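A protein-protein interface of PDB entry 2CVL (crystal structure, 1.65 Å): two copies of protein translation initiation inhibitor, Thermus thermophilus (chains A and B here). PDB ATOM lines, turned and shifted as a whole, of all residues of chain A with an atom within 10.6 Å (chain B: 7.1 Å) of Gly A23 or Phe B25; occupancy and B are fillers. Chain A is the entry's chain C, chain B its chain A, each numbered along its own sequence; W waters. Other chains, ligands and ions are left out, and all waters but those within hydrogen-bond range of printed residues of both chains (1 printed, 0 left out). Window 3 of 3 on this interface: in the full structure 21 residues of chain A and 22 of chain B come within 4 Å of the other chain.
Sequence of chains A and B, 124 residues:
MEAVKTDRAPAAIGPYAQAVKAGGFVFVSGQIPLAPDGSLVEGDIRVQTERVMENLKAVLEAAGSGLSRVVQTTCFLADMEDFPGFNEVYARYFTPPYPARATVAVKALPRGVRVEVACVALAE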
ATOM      1  N   MET A   1      -7.634  20.655 -22.378  1.00  0.00           N
ATOM      2  CA  MET A   1      -9.118  20.719 -22.512  1.00  0.00           C
ATOM      3  C   MET A   1      -9.728  19.322 -22.588  1.00  0.00           C
ATOM      4  O   MET A   1      -9.069  18.370 -23.005  1.00  0.00           O
ATOM      5  CB  MET A   1      -9.492  21.509 -23.763  1.00  0.00           C
ATOM      6  CG  MET A   1      -8.819  21.007 -25.026  1.00  0.00           C
ATOM      7  SD  MET A   1      -9.467  21.959 -26.569  1.00  0.00           S
ATOM      8  CE  MET A   1     -10.837  20.722 -27.127  1.00  0.00           C
ATOM      9  N   GLU A   2     -10.990  19.209 -22.189  1.00  0.00           N
ATOM     10  CA  GLU A   2     -11.681  17.923 -22.201  1.00  0.00           C
ATOM     11  C   GLU A   2     -12.916  17.955 -23.092  1.00  0.00           C
ATOM     12  O   GLU A   2     -13.817  18.770 -22.893  1.00  0.00           O
ATOM     13  CB  GLU A   2     -12.082  17.540 -20.773  1.00  0.00           C
ATOM     14  CG  GLU A   2     -12.844  16.230 -20.658  1.00  0.00           C
ATOM     15  CD  GLU A   2     -13.232  15.911 -19.226  1.00  0.00           C
ATOM     16  OE1 GLU A   2     -13.914  16.742 -18.592  1.00  0.00           O
ATOM     17  OE2 GLU A   2     -12.853  14.828 -18.732  1.00  0.00           O
ATOM     18  N   VAL A  20     -16.679  21.524 -25.061  1.00  0.00           N
ATOM     19  CA  VAL A  20     -15.348  21.393 -24.488  1.00  0.00           C
ATOM     20  C   VAL A  20     -15.348  22.009 -23.101  1.00  0.00           C
ATOM     21  O   VAL A  20     -15.890  23.094 -22.904  1.00  0.00           O
ATOM     22  CB  VAL A  20     -14.288  22.125 -25.344  1.00  0.00           C
ATOM     23  CG1 VAL A  20     -12.951  22.147 -24.613  1.00  0.00           C
ATOM     24  CG2 VAL A  20     -14.141  21.437 -26.689  1.00  0.00           C
ATOM     25  N   LYS A  21     -14.751  21.306 -22.140  1.00  0.00           N
ATOM     26  CA  LYS A  21     -14.658  21.814 -20.779  1.00  0.00           C
ATOM     27  C   LYS A  21     -13.265  22.403 -20.611  1.00  0.00           C
ATOM     28  O   LYS A  21     -12.263  21.725 -20.855  1.00  0.00           O
ATOM     29  CB  LYS A  21     -14.871  20.690 -19.761  1.00  0.00           C
ATOM     30  CG  LYS A  21     -16.248  20.048 -19.824  1.00  0.00           C
ATOM     31  CD  LYS A  21     -16.421  18.971 -18.759  1.00  0.00           C
ATOM     32  CE  LYS A  21     -16.345  19.553 -17.357  1.00  0.00           C
ATOM     33  NZ  LYS A  21     -16.608  18.517 -16.318  1.00  0.00           N
ATOM     34  N   ALA A  22     -13.203  23.668 -20.215  1.00  0.00           N
ATOM     35  CA  ALA A  22     -11.920  24.331 -20.035  1.00  0.00           C
ATOM     36  C   ALA A  22     -12.014  25.630 -19.247  1.00  0.00           C
ATOM     37  O   ALA A  22     -12.957  26.406 -19.407  1.00  0.00           O
ATOM     38  CB  ALA A  22     -11.282  24.600 -21.397  1.00  0.00           C
ATOM     39  N   GLY A  23     -11.022  25.854 -18.393  1.00  0.00           N
ATOM     40  CA  GLY A  23     -10.976  27.071 -17.603  1.00  0.00           C
ATOM     41  C   GLY A  23     -12.175  27.358 -16.722  1.00  0.00           C
ATOM     42  O   GLY A  23     -12.442  28.516 -16.408  1.00  0.00           O
ATOM     43  N   GLY A  24     -12.896  26.317 -16.323  1.00  0.00           N
ATOM     44  CA  GLY A  24     -14.051  26.508 -15.464  1.00  0.00           C
ATOM     45  C   GLY A  24     -15.345  26.705 -16.233  1.00  0.00           C
ATOM     46  O   GLY A  24     -16.413  26.872 -15.640  1.00  0.00           O
ATOM     47  N   PHE A  25     -15.248  26.679 -17.555  1.00  0.00           N
ATOM     48  CA  PHE A  25     -16.423  26.853 -18.399  1.00  0.00           C
ATOM     49  C   PHE A  25     -16.649  25.650 -19.301  1.00  0.00           C
ATOM     50  O   PHE A  25     -15.803  24.757 -19.411  1.00  0.00           O
ATOM     51  CB  PHE A  25     -16.282  28.098 -19.286  1.00  0.00           C
ATOM     52  CG  PHE A  25     -16.263  29.399 -18.528  1.00  0.00           C
ATOM     53  CD1 PHE A  25     -15.061  30.051 -18.270  1.00  0.00           C
ATOM     54  CD2 PHE A  25     -17.451  29.982 -18.091  1.00  0.00           C
ATOM     55  CE1 PHE A  25     -15.037  31.273 -17.587  1.00  0.00           C
ATOM     56  CE2 PHE A  25     -17.441  31.201 -17.406  1.00  0.00           C
ATOM     57  CZ  PHE A  25     -16.231  31.848 -17.155  1.00  0.00           C
ATOM     58  N   VAL A  26     -17.812  25.638 -19.937  1.00  0.00           N
ATOM     59  CA  VAL A  26     -18.173  24.593 -20.882  1.00  0.00           C
ATOM     60  C   VAL A  26     -18.533  25.365 -22.139  1.00  0.00           C
ATOM     61  O   VAL A  26     -19.451  26.187 -22.129  1.00  0.00           O
ATOM     62  CB  VAL A  26     -19.402  23.779 -20.415  1.00  0.00           C
ATOM     63  CG1 VAL A  26     -19.761  22.718 -21.460  1.00  0.00           C
ATOM     64  CG2 VAL A  26     -19.110  23.125 -19.067  1.00  0.00           C
ATOM     65  N   PHE A  27     -17.776  25.133 -23.205  1.00  0.00           N
ATOM     66  CA  PHE A  27     -18.021  25.798 -24.475  1.00  0.00           C
ATOM     67  C   PHE A  27     -18.801  24.813 -25.337  1.00  0.00           C
ATOM     68  O   PHE A  27     -18.290  23.756 -25.704  1.00  0.00           O
ATOM     69  CB  PHE A  27     -16.690  26.169 -25.136  1.00  0.00           C
ATOM     70  CG  PHE A  27     -15.880  27.161 -24.344  1.00  0.00           C
ATOM     71  CD1 PHE A  27     -15.993  28.526 -24.590  1.00  0.00           C
ATOM     72  CD2 PHE A  27     -15.039  26.734 -23.320  1.00  0.00           C
ATOM     73  CE1 PHE A  27     -15.285  29.450 -23.830  1.00  0.00           C
ATOM     74  CE2 PHE A  27     -14.326  27.653 -22.552  1.00  0.00           C
ATOM     75  CZ  PHE A  27     -14.450  29.010 -22.806  1.00  0.00           C
ATOM     76  N   ARG A  69     -26.874  26.871 -15.703  1.00  0.00           N
ATOM     77  CA  ARG A  69     -25.485  27.295 -15.559  1.00  0.00           C
ATOM     78  C   ARG A  69     -24.977  28.056 -16.781  1.00  0.00           C
ATOM     79  O   ARG A  69     -23.833  28.514 -16.804  1.00  0.00           O
ATOM     80  CB  ARG A  69     -24.595  26.076 -15.303  1.00  0.00           C
ATOM     81  CG  ARG A  69     -25.025  25.242 -14.107  1.00  0.00           C
ATOM     82  CD  ARG A  69     -24.689  25.927 -12.794  1.00  0.00           C
ATOM     83  NE  ARG A  69     -23.254  25.899 -12.522  1.00  0.00           N
ATOM     84  CZ  ARG A  69     -22.685  26.430 -11.445  1.00  0.00           C
ATOM     85  NH1 ARG A  69     -23.427  27.039 -10.530  1.00  0.00           N
ATOM     86  NH2 ARG A  69     -21.373  26.349 -11.280  1.00  0.00           N
ATOM     87  N   VAL A  71     -24.208  30.987 -19.055  1.00  0.00           N
ATOM     88  CA  VAL A  71     -23.990  32.406 -18.806  1.00  0.00           C
ATOM     89  C   VAL A  71     -24.021  33.257 -20.073  1.00  0.00           C
ATOM     90  O   VAL A  71     -24.136  34.482 -20.007  1.00  0.00           O
ATOM     91  CB  VAL A  71     -22.637  32.645 -18.085  1.00  0.00           C
ATOM     92  CG1 VAL A  71     -22.616  31.895 -16.767  1.00  0.00           C
ATOM     93  CG2 VAL A  71     -21.476  32.190 -18.968  1.00  0.00           C
ATOM     94  N   VAL A 120     -22.018  29.222 -23.684  1.00  0.00           N
ATOM     95  CA  VAL A 120     -20.929  29.058 -22.740  1.00  0.00           C
ATOM     96  C   VAL A 120     -21.604  28.952 -21.378  1.00  0.00           C
ATOM     97  O   VAL A 120     -22.468  29.763 -21.034  1.00  0.00           O
ATOM     98  CB  VAL A 120     -19.978  30.266 -22.762  1.00  0.00           C
ATOM     99  CG1 VAL A 120     -18.950  30.132 -21.651  1.00  0.00           C
ATOM    100  CG2 VAL A 120     -19.285  30.353 -24.119  1.00  0.00           C
ATOM    101  N   ALA A 121     -21.230  27.936 -20.612  1.00  0.00           N
ATOM    102  CA  ALA A 121     -21.819  27.732 -19.300  1.00  0.00           C
ATOM    103  C   ALA A 121     -20.740  27.490 -18.259  1.00  0.00           C
ATOM    104  O   ALA A 121     -19.588  27.233 -18.596  1.00  0.00           O
ATOM    105  CB  ALA A 121     -22.769  26.541 -19.340  1.00  0.00           C
ATOM    106  N   LEU A 122     -21.121  27.593 -16.991  1.00  0.00           N
ATOM    107  CA  LEU A 122     -20.187  27.338 -15.906  1.00  0.00           C
ATOM    108  C   LEU A 122     -20.055  25.830 -15.750  1.00  0.00           C
ATOM    109  O   LEU A 122     -21.034  25.093 -15.887  1.00  0.00           O
ATOM    110  CB  LEU A 122     -20.700  27.957 -14.605  1.00  0.00           C
ATOM    111  CG  LEU A 122     -20.552  29.475 -14.481  1.00  0.00           C
ATOM    112  CD1 LEU A 122     -21.377  29.981 -13.307  1.00  0.00           C
ATOM    113  CD2 LEU A 122     -19.080  29.831 -14.302  1.00  0.00           C
ATOM    114  N   ALA A 123     -18.838  25.370 -15.479  1.00  0.00           N
ATOM    115  CA  ALA A 123     -18.594  23.946 -15.303  1.00  0.00           C
ATOM    116  C   ALA A 123     -19.070  23.529 -13.919  1.00  0.00           C
ATOM    117  O   ALA A 123     -19.450  24.375 -13.109  1.00  0.00           O
ATOM    118  CB  ALA A 123     -17.107  23.648 -15.462  1.00  0.00           C
ATOM    119  N   GLU A 124     -19.052  22.226 -13.656  1.00  0.00           N
ATOM    120  CA  GLU A 124     -19.470  21.695 -12.360  1.00  0.00           C
ATOM    121  C   GLU A 124     -20.985  21.743 -12.205  1.00  0.00           C
ATOM    122  O   GLU A 124     -21.579  20.679 -11.929  1.00  0.00           O
ATOM    123  CB  GLU A 124     -18.811  22.493 -11.232  1.00  0.00           C
ATOM    124  CG  GLU A 124     -17.310  22.652 -11.392  1.00  0.00           C
ATOM    125  CD  GLU A 124     -16.765  23.826 -10.609  1.00  0.00           C
ATOM    126  OE1 GLU A 124     -16.859  23.808  -9.365  1.00  0.00           O
ATOM    127  OE2 GLU A 124     -16.248  24.772 -11.244  1.00  0.00           O
ATOM    128  OXT GLU A 124     -21.558  22.845 -12.355  1.00  0.00           O
ATOM    129  N   VAL B  20      -5.945  38.973 -27.233  1.00  0.00           N
ATOM    130  CA  VAL B  20      -5.806  39.492 -25.882  1.00  0.00           C
ATOM    131  C   VAL B  20      -5.707  38.331 -24.905  1.00  0.00           C
ATOM    132  O   VAL B  20      -6.478  37.374 -24.985  1.00  0.00           O
ATOM    133  CB  VAL B  20      -7.018  40.364 -25.473  1.00  0.00           C
ATOM    134  CG1 VAL B  20      -6.927  40.707 -23.991  1.00  0.00           C
ATOM    135  CG2 VAL B  20      -7.058  41.636 -26.308  1.00  0.00           C
ATOM    136  N   LYS B  21      -4.746  38.415 -23.989  1.00  0.00           N
ATOM    137  CA  LYS B  21      -4.563  37.386 -22.975  1.00  0.00           C
ATOM    138  C   LYS B  21      -5.219  37.915 -21.705  1.00  0.00           C
ATOM    139  O   LYS B  21      -4.901  39.018 -21.254  1.00  0.00           O
ATOM    140  CB  LYS B  21      -3.071  37.139 -22.722  1.00  0.00           C
ATOM    141  CG  LYS B  21      -2.295  36.677 -23.944  1.00  0.00           C
ATOM    142  CD  LYS B  21      -0.805  36.513 -23.651  1.00  0.00           C
ATOM    143  CE  LYS B  21      -0.545  35.403 -22.653  1.00  0.00           C
ATOM    144  NZ  LYS B  21       0.913  35.189 -22.448  1.00  0.00           N
ATOM    145  N   ALA B  22      -6.142  37.143 -21.144  1.00  0.00           N
ATOM    146  CA  ALA B  22      -6.828  37.557 -19.926  1.00  0.00           C
ATOM    147  C   ALA B  22      -7.648  36.437 -19.294  1.00  0.00           C
ATOM    148  O   ALA B  22      -8.230  35.603 -19.987  1.00  0.00           O
ATOM    149  CB  ALA B  22      -7.729  38.758 -20.221  1.00  0.00           C
ATOM    150  N   GLY B  23      -7.684  36.426 -17.966  1.00  0.00           N
ATOM    151  CA  GLY B  23      -8.450  35.423 -17.247  1.00  0.00           C
ATOM    152  C   GLY B  23      -8.104  33.974 -17.542  1.00  0.00           C
ATOM    153  O   GLY B  23      -8.933  33.088 -17.350  1.00  0.00           O
ATOM    154  N   GLY B  24      -6.881  33.726 -18.001  1.00  0.00           N
ATOM    155  CA  GLY B  24      -6.474  32.367 -18.303  1.00  0.00           C
ATOM    156  C   GLY B  24      -6.807  31.939 -19.719  1.00  0.00           C
ATOM    157  O   GLY B  24      -6.589  30.788 -20.094  1.00  0.00           O
ATOM    158  N   PHE B  25      -7.337  32.867 -20.507  1.00  0.00           N
ATOM    159  CA  PHE B  25      -7.692  32.574 -21.892  1.00  0.00           C
ATOM    160  C   PHE B  25      -7.014  33.540 -22.844  1.00  0.00           C
ATOM    161  O   PHE B  25      -6.447  34.550 -22.429  1.00  0.00           O
ATOM    162  CB  PHE B  25      -9.206  32.689 -22.119  1.00  0.00           C
ATOM    163  CG  PHE B  25     -10.015  31.618 -21.453  1.00  0.00           C
ATOM    164  CD1 PHE B  25     -10.566  31.823 -20.194  1.00  0.00           C
ATOM    165  CD2 PHE B  25     -10.242  30.401 -22.094  1.00  0.00           C
ATOM    166  CE1 PHE B  25     -11.336  30.835 -19.585  1.00  0.00           C
ATOM    167  CE2 PHE B  25     -11.006  29.412 -21.492  1.00  0.00           C
ATOM    168  CZ  PHE B  25     -11.557  29.628 -20.236  1.00  0.00           C
ATOM    169  N   VAL B  26      -7.074  33.205 -24.130  1.00  0.00           N
ATOM    170  CA  VAL B  26      -6.539  34.051 -25.180  1.00  0.00           C
ATOM    171  C   VAL B  26      -7.711  34.246 -26.121  1.00  0.00           C
ATOM    172  O   VAL B  26      -8.265  33.279 -26.641  1.00  0.00           O
ATOM    173  CB  VAL B  26      -5.399  33.389 -25.969  1.00  0.00           C
ATOM    174  CG1 VAL B  26      -4.930  34.335 -27.078  1.00  0.00           C
ATOM    175  CG2 VAL B  26      -4.238  33.063 -25.042  1.00  0.00           C
ATOM    176  N   PHE B  27      -8.103  35.498 -26.311  1.00  0.00           N
ATOM    177  CA  PHE B  27      -9.209  35.827 -27.193  1.00  0.00           C
ATOM    178  C   PHE B  27      -8.585  36.318 -28.491  1.00  0.00           C
ATOM    179  O   PHE B  27      -7.841  37.299 -28.500  1.00  0.00           O
ATOM    180  CB  PHE B  27     -10.068  36.907 -26.541  1.00  0.00           C
ATOM    181  CG  PHE B  27     -10.674  36.477 -25.237  1.00  0.00           C
ATOM    182  CD1 PHE B  27     -11.927  35.875 -25.203  1.00  0.00           C
ATOM    183  CD2 PHE B  27      -9.972  36.630 -24.042  1.00  0.00           C
ATOM    184  CE1 PHE B  27     -12.473  35.430 -24.002  1.00  0.00           C
ATOM    185  CE2 PHE B  27     -10.510  36.187 -22.834  1.00  0.00           C
ATOM    186  CZ  PHE B  27     -11.763  35.586 -22.814  1.00  0.00           C
ATOM    187  N   ARG B  69      -4.729  24.317 -27.943  1.00  0.00           N
ATOM    188  CA  ARG B  69      -5.319  24.919 -26.749  1.00  0.00           C
ATOM    189  C   ARG B  69      -6.616  25.644 -27.084  1.00  0.00           C
ATOM    190  O   ARG B  69      -7.276  26.190 -26.198  1.00  0.00           O
ATOM    191  CB  ARG B  69      -4.331  25.903 -26.113  1.00  0.00           C
ATOM    192  CG  ARG B  69      -2.998  25.282 -25.717  1.00  0.00           C
ATOM    193  CD  ARG B  69      -2.919  25.016 -24.224  1.00  0.00           C
ATOM    194  NE  ARG B  69      -3.886  24.026 -23.766  1.00  0.00           N
ATOM    195  CZ  ARG B  69      -4.087  23.718 -22.488  1.00  0.00           C
ATOM    196  NH1 ARG B  69      -3.389  24.329 -21.539  1.00  0.00           N
ATOM    197  NH2 ARG B  69      -4.985  22.800 -22.159  1.00  0.00           N
ATOM    198  N   VAL B  71     -10.348  26.232 -27.633  1.00  0.00           N
ATOM    199  CA  VAL B  71     -11.543  25.599 -27.083  1.00  0.00           C
ATOM    200  C   VAL B  71     -12.826  25.986 -27.805  1.00  0.00           C
ATOM    201  O   VAL B  71     -13.846  25.314 -27.672  1.00  0.00           O
ATOM    202  CB  VAL B  71     -11.719  25.954 -25.585  1.00  0.00           C
ATOM    203  CG1 VAL B  71     -10.513  25.483 -24.793  1.00  0.00           C
ATOM    204  CG2 VAL B  71     -11.898  27.463 -25.421  1.00  0.00           C
ATOM    205  N   VAL B 120     -11.182  31.299 -29.281  1.00  0.00           N
ATOM    206  CA  VAL B 120     -10.812  31.488 -27.884  1.00  0.00           C
ATOM    207  C   VAL B 120     -10.027  30.242 -27.512  1.00  0.00           C
ATOM    208  O   VAL B 120     -10.413  29.135 -27.881  1.00  0.00           O
ATOM    209  CB  VAL B 120     -12.053  31.597 -26.969  1.00  0.00           C
ATOM    210  CG1 VAL B 120     -11.625  31.666 -25.504  1.00  0.00           C
ATOM    211  CG2 VAL B 120     -12.854  32.834 -27.334  1.00  0.00           C
ATOM    212  N   ALA B 121      -8.926  30.424 -26.794  1.00  0.00           N
ATOM    213  CA  ALA B 121      -8.093  29.302 -26.388  1.00  0.00           C
ATOM    214  C   ALA B 121      -7.613  29.486 -24.958  1.00  0.00           C
ATOM    215  O   ALA B 121      -7.738  30.565 -24.384  1.00  0.00           O
ATOM    216  CB  ALA B 121      -6.900  29.189 -27.320  1.00  0.00           C
ATOM    217  N   LEU B 122      -7.085  28.414 -24.380  1.00  0.00           N
ATOM    218  CA  LEU B 122      -6.546  28.470 -23.028  1.00  0.00           C
ATOM    219  C   LEU B 122      -5.157  29.082 -23.149  1.00  0.00           C
ATOM    220  O   LEU B 122      -4.453  28.841 -24.127  1.00  0.00           O
ATOM    221  CB  LEU B 122      -6.441  27.064 -22.434  1.00  0.00           C
ATOM    222  CG  LEU B 122      -7.748  26.420 -21.965  1.00  0.00           C
ATOM    223  CD1 LEU B 122      -7.541  24.932 -21.731  1.00  0.00           C
ATOM    224  CD2 LEU B 122      -8.220  27.109 -20.693  1.00  0.00           C
ATOM    225  N   ALA B 123      -4.766  29.877 -22.159  1.00  0.00           N
ATOM    226  CA  ALA B 123      -3.456  30.518 -22.181  1.00  0.00           C
ATOM    227  C   ALA B 123      -2.356  29.559 -21.734  1.00  0.00           C
ATOM    228  O   ALA B 123      -1.201  29.958 -21.583  1.00  0.00           O
ATOM    229  CB  ALA B 123      -3.466  31.754 -21.287  1.00  0.00           C
ATOM    230  N   GLU B 124      -2.722  28.297 -21.532  1.00  0.00           N
ATOM    231  CA  GLU B 124      -1.783  27.267 -21.088  1.00  0.00           C
ATOM    232  C   GLU B 124      -1.420  27.485 -19.623  1.00  0.00           C
ATOM    233  O   GLU B 124      -0.241  27.790 -19.347  1.00  0.00           O
ATOM    234  CB  GLU B 124      -0.502  27.278 -21.934  1.00  0.00           C
ATOM    235  CG  GLU B 124      -0.725  27.103 -23.426  1.00  0.00           C
ATOM    236  CD  GLU B 124       0.437  26.409 -24.114  1.00  0.00           C
ATOM    237  OE1 GLU B 124       0.712  25.237 -23.779  1.00  0.00           O
ATOM    238  OE2 GLU B 124       1.075  27.032 -24.988  1.00  0.00           O
ATOM    239  OXT GLU B 124      -2.324  27.355 -18.771  1.00  0.00           O
HETATM  240  O   HOH W   1      -9.507  30.324 -16.672  1.00  0.00           O
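NH2 of Arg B69 sits close to N of Met A1 (3.4 Å).
N of Val B71 is in hydrogen-bond range of O of Val B120.
O of Val A20 lies within hydrogen-bond range of N of Phe A27, at 2.8 Å.
The backbone NH (N) of Leu B122 sits at hydrogen-bond distance from the backbone carbonyl oxygen (O) of Arg B69, at 2.9 Å.
O of Val B71 touches CB of Val A20, at 3.97 Å.
Ala A22 touches Phe B25 (O to CZ, 3.6 Å).
Ala A22 touches Val B71.
Leu B122 touches Ala A22.
CA of Gly A23 touches CZ of Phe B25, 3.7 Å away.
N of Gly A23 touches CD2 of Leu B122, at 3.8 Å.
Phe B25 touches Phe A27.
Phe A27 touches Val B71 (CE2 to CG2, 3.8 Å).
Gly A23 touches just these residues of chain B: Phe B25 (3.7 Å) and Leu B122 (3.8 Å).
Of chain A, only Ala A22 (3.6 Å), Gly A23 (3.7 Å) and Phe A27 (3.7 Å) come within 4 Å of Phe B25.
Ala B22 touches none of the printed residues of chain A.
No residue of chain A comes within 4 Å of Gly B24.
No residue of chain A comes within 4 Å of Val B26.
Of chain A, only Ala A22 (3.8 Å) and Gly A23 (3.8 Å) come within 4 Å of Leu B122.
Printed residues of chain B within 4 Å of Ala A22: Phe B25 (3.6 Å), Val B71 (3.6 Å) and Leu B122 (3.8 Å).
Printed residues of chain B within 4 Å of Val A20: Val B71 (3.97 Å).
Of the printed residues of chain A, Arg B69 touches Met A1 (3.4 Å).
Of the printed residues of chain B, Met A1 touches Arg B69 (3.4 Å).
Of the printed residues of chain A, Val B71 touches Val A20, Ala A22 and Phe A27.
Ala A121 touches none of the printed residues of chain B.
Glu A2 touches none of the printed residues of chain B.
Printed residues of chain B that touch a printed residue of chain A: Phe B25, Arg B69, Val B71 and Leu B122.
Hydrophobic or aromatic side chains of chain B that line the printed part of chain A: Phe B25, Val B71 and Leu B122.
Along chain B the printed residues that touch a printed residue of chain A span positions 25 to 122.
Of the 17 printed residues of chain A, 5 touch a printed residue of chain B.
Val A20 touches Val B71, but with the chains exchanged Val A71 does not touch Val B20 (17.0 Å).
Ala A22 touches Phe B25, but with the chains exchanged Phe A25 does not touch Ala B22 (8.4 Å).
Ala A22 touches Val B71, but with the chains exchanged Val A71 does not touch Ala B22 (13.7 Å).
Gly A23 touches Phe B25, but with the chains exchanged Phe A25 does not touch Gly B23 (6.4 Å).
Positions printed for both chains: 20, 21, 22, 23, 24, 25, 26, 27, 69, 71, 120, 121, 122, 123 and 124.
Of the 9 pairs that touch across the chains among the printed residues, none has its exchanged pair printed and touching as well.
Water W1 lies within hydrogen-bond range of the backbone carbonyl oxygen (O) of Gly B23 (2.9 Å) and the backbone carbonyl oxygen (O) of Gly A23 (3.5 Å).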
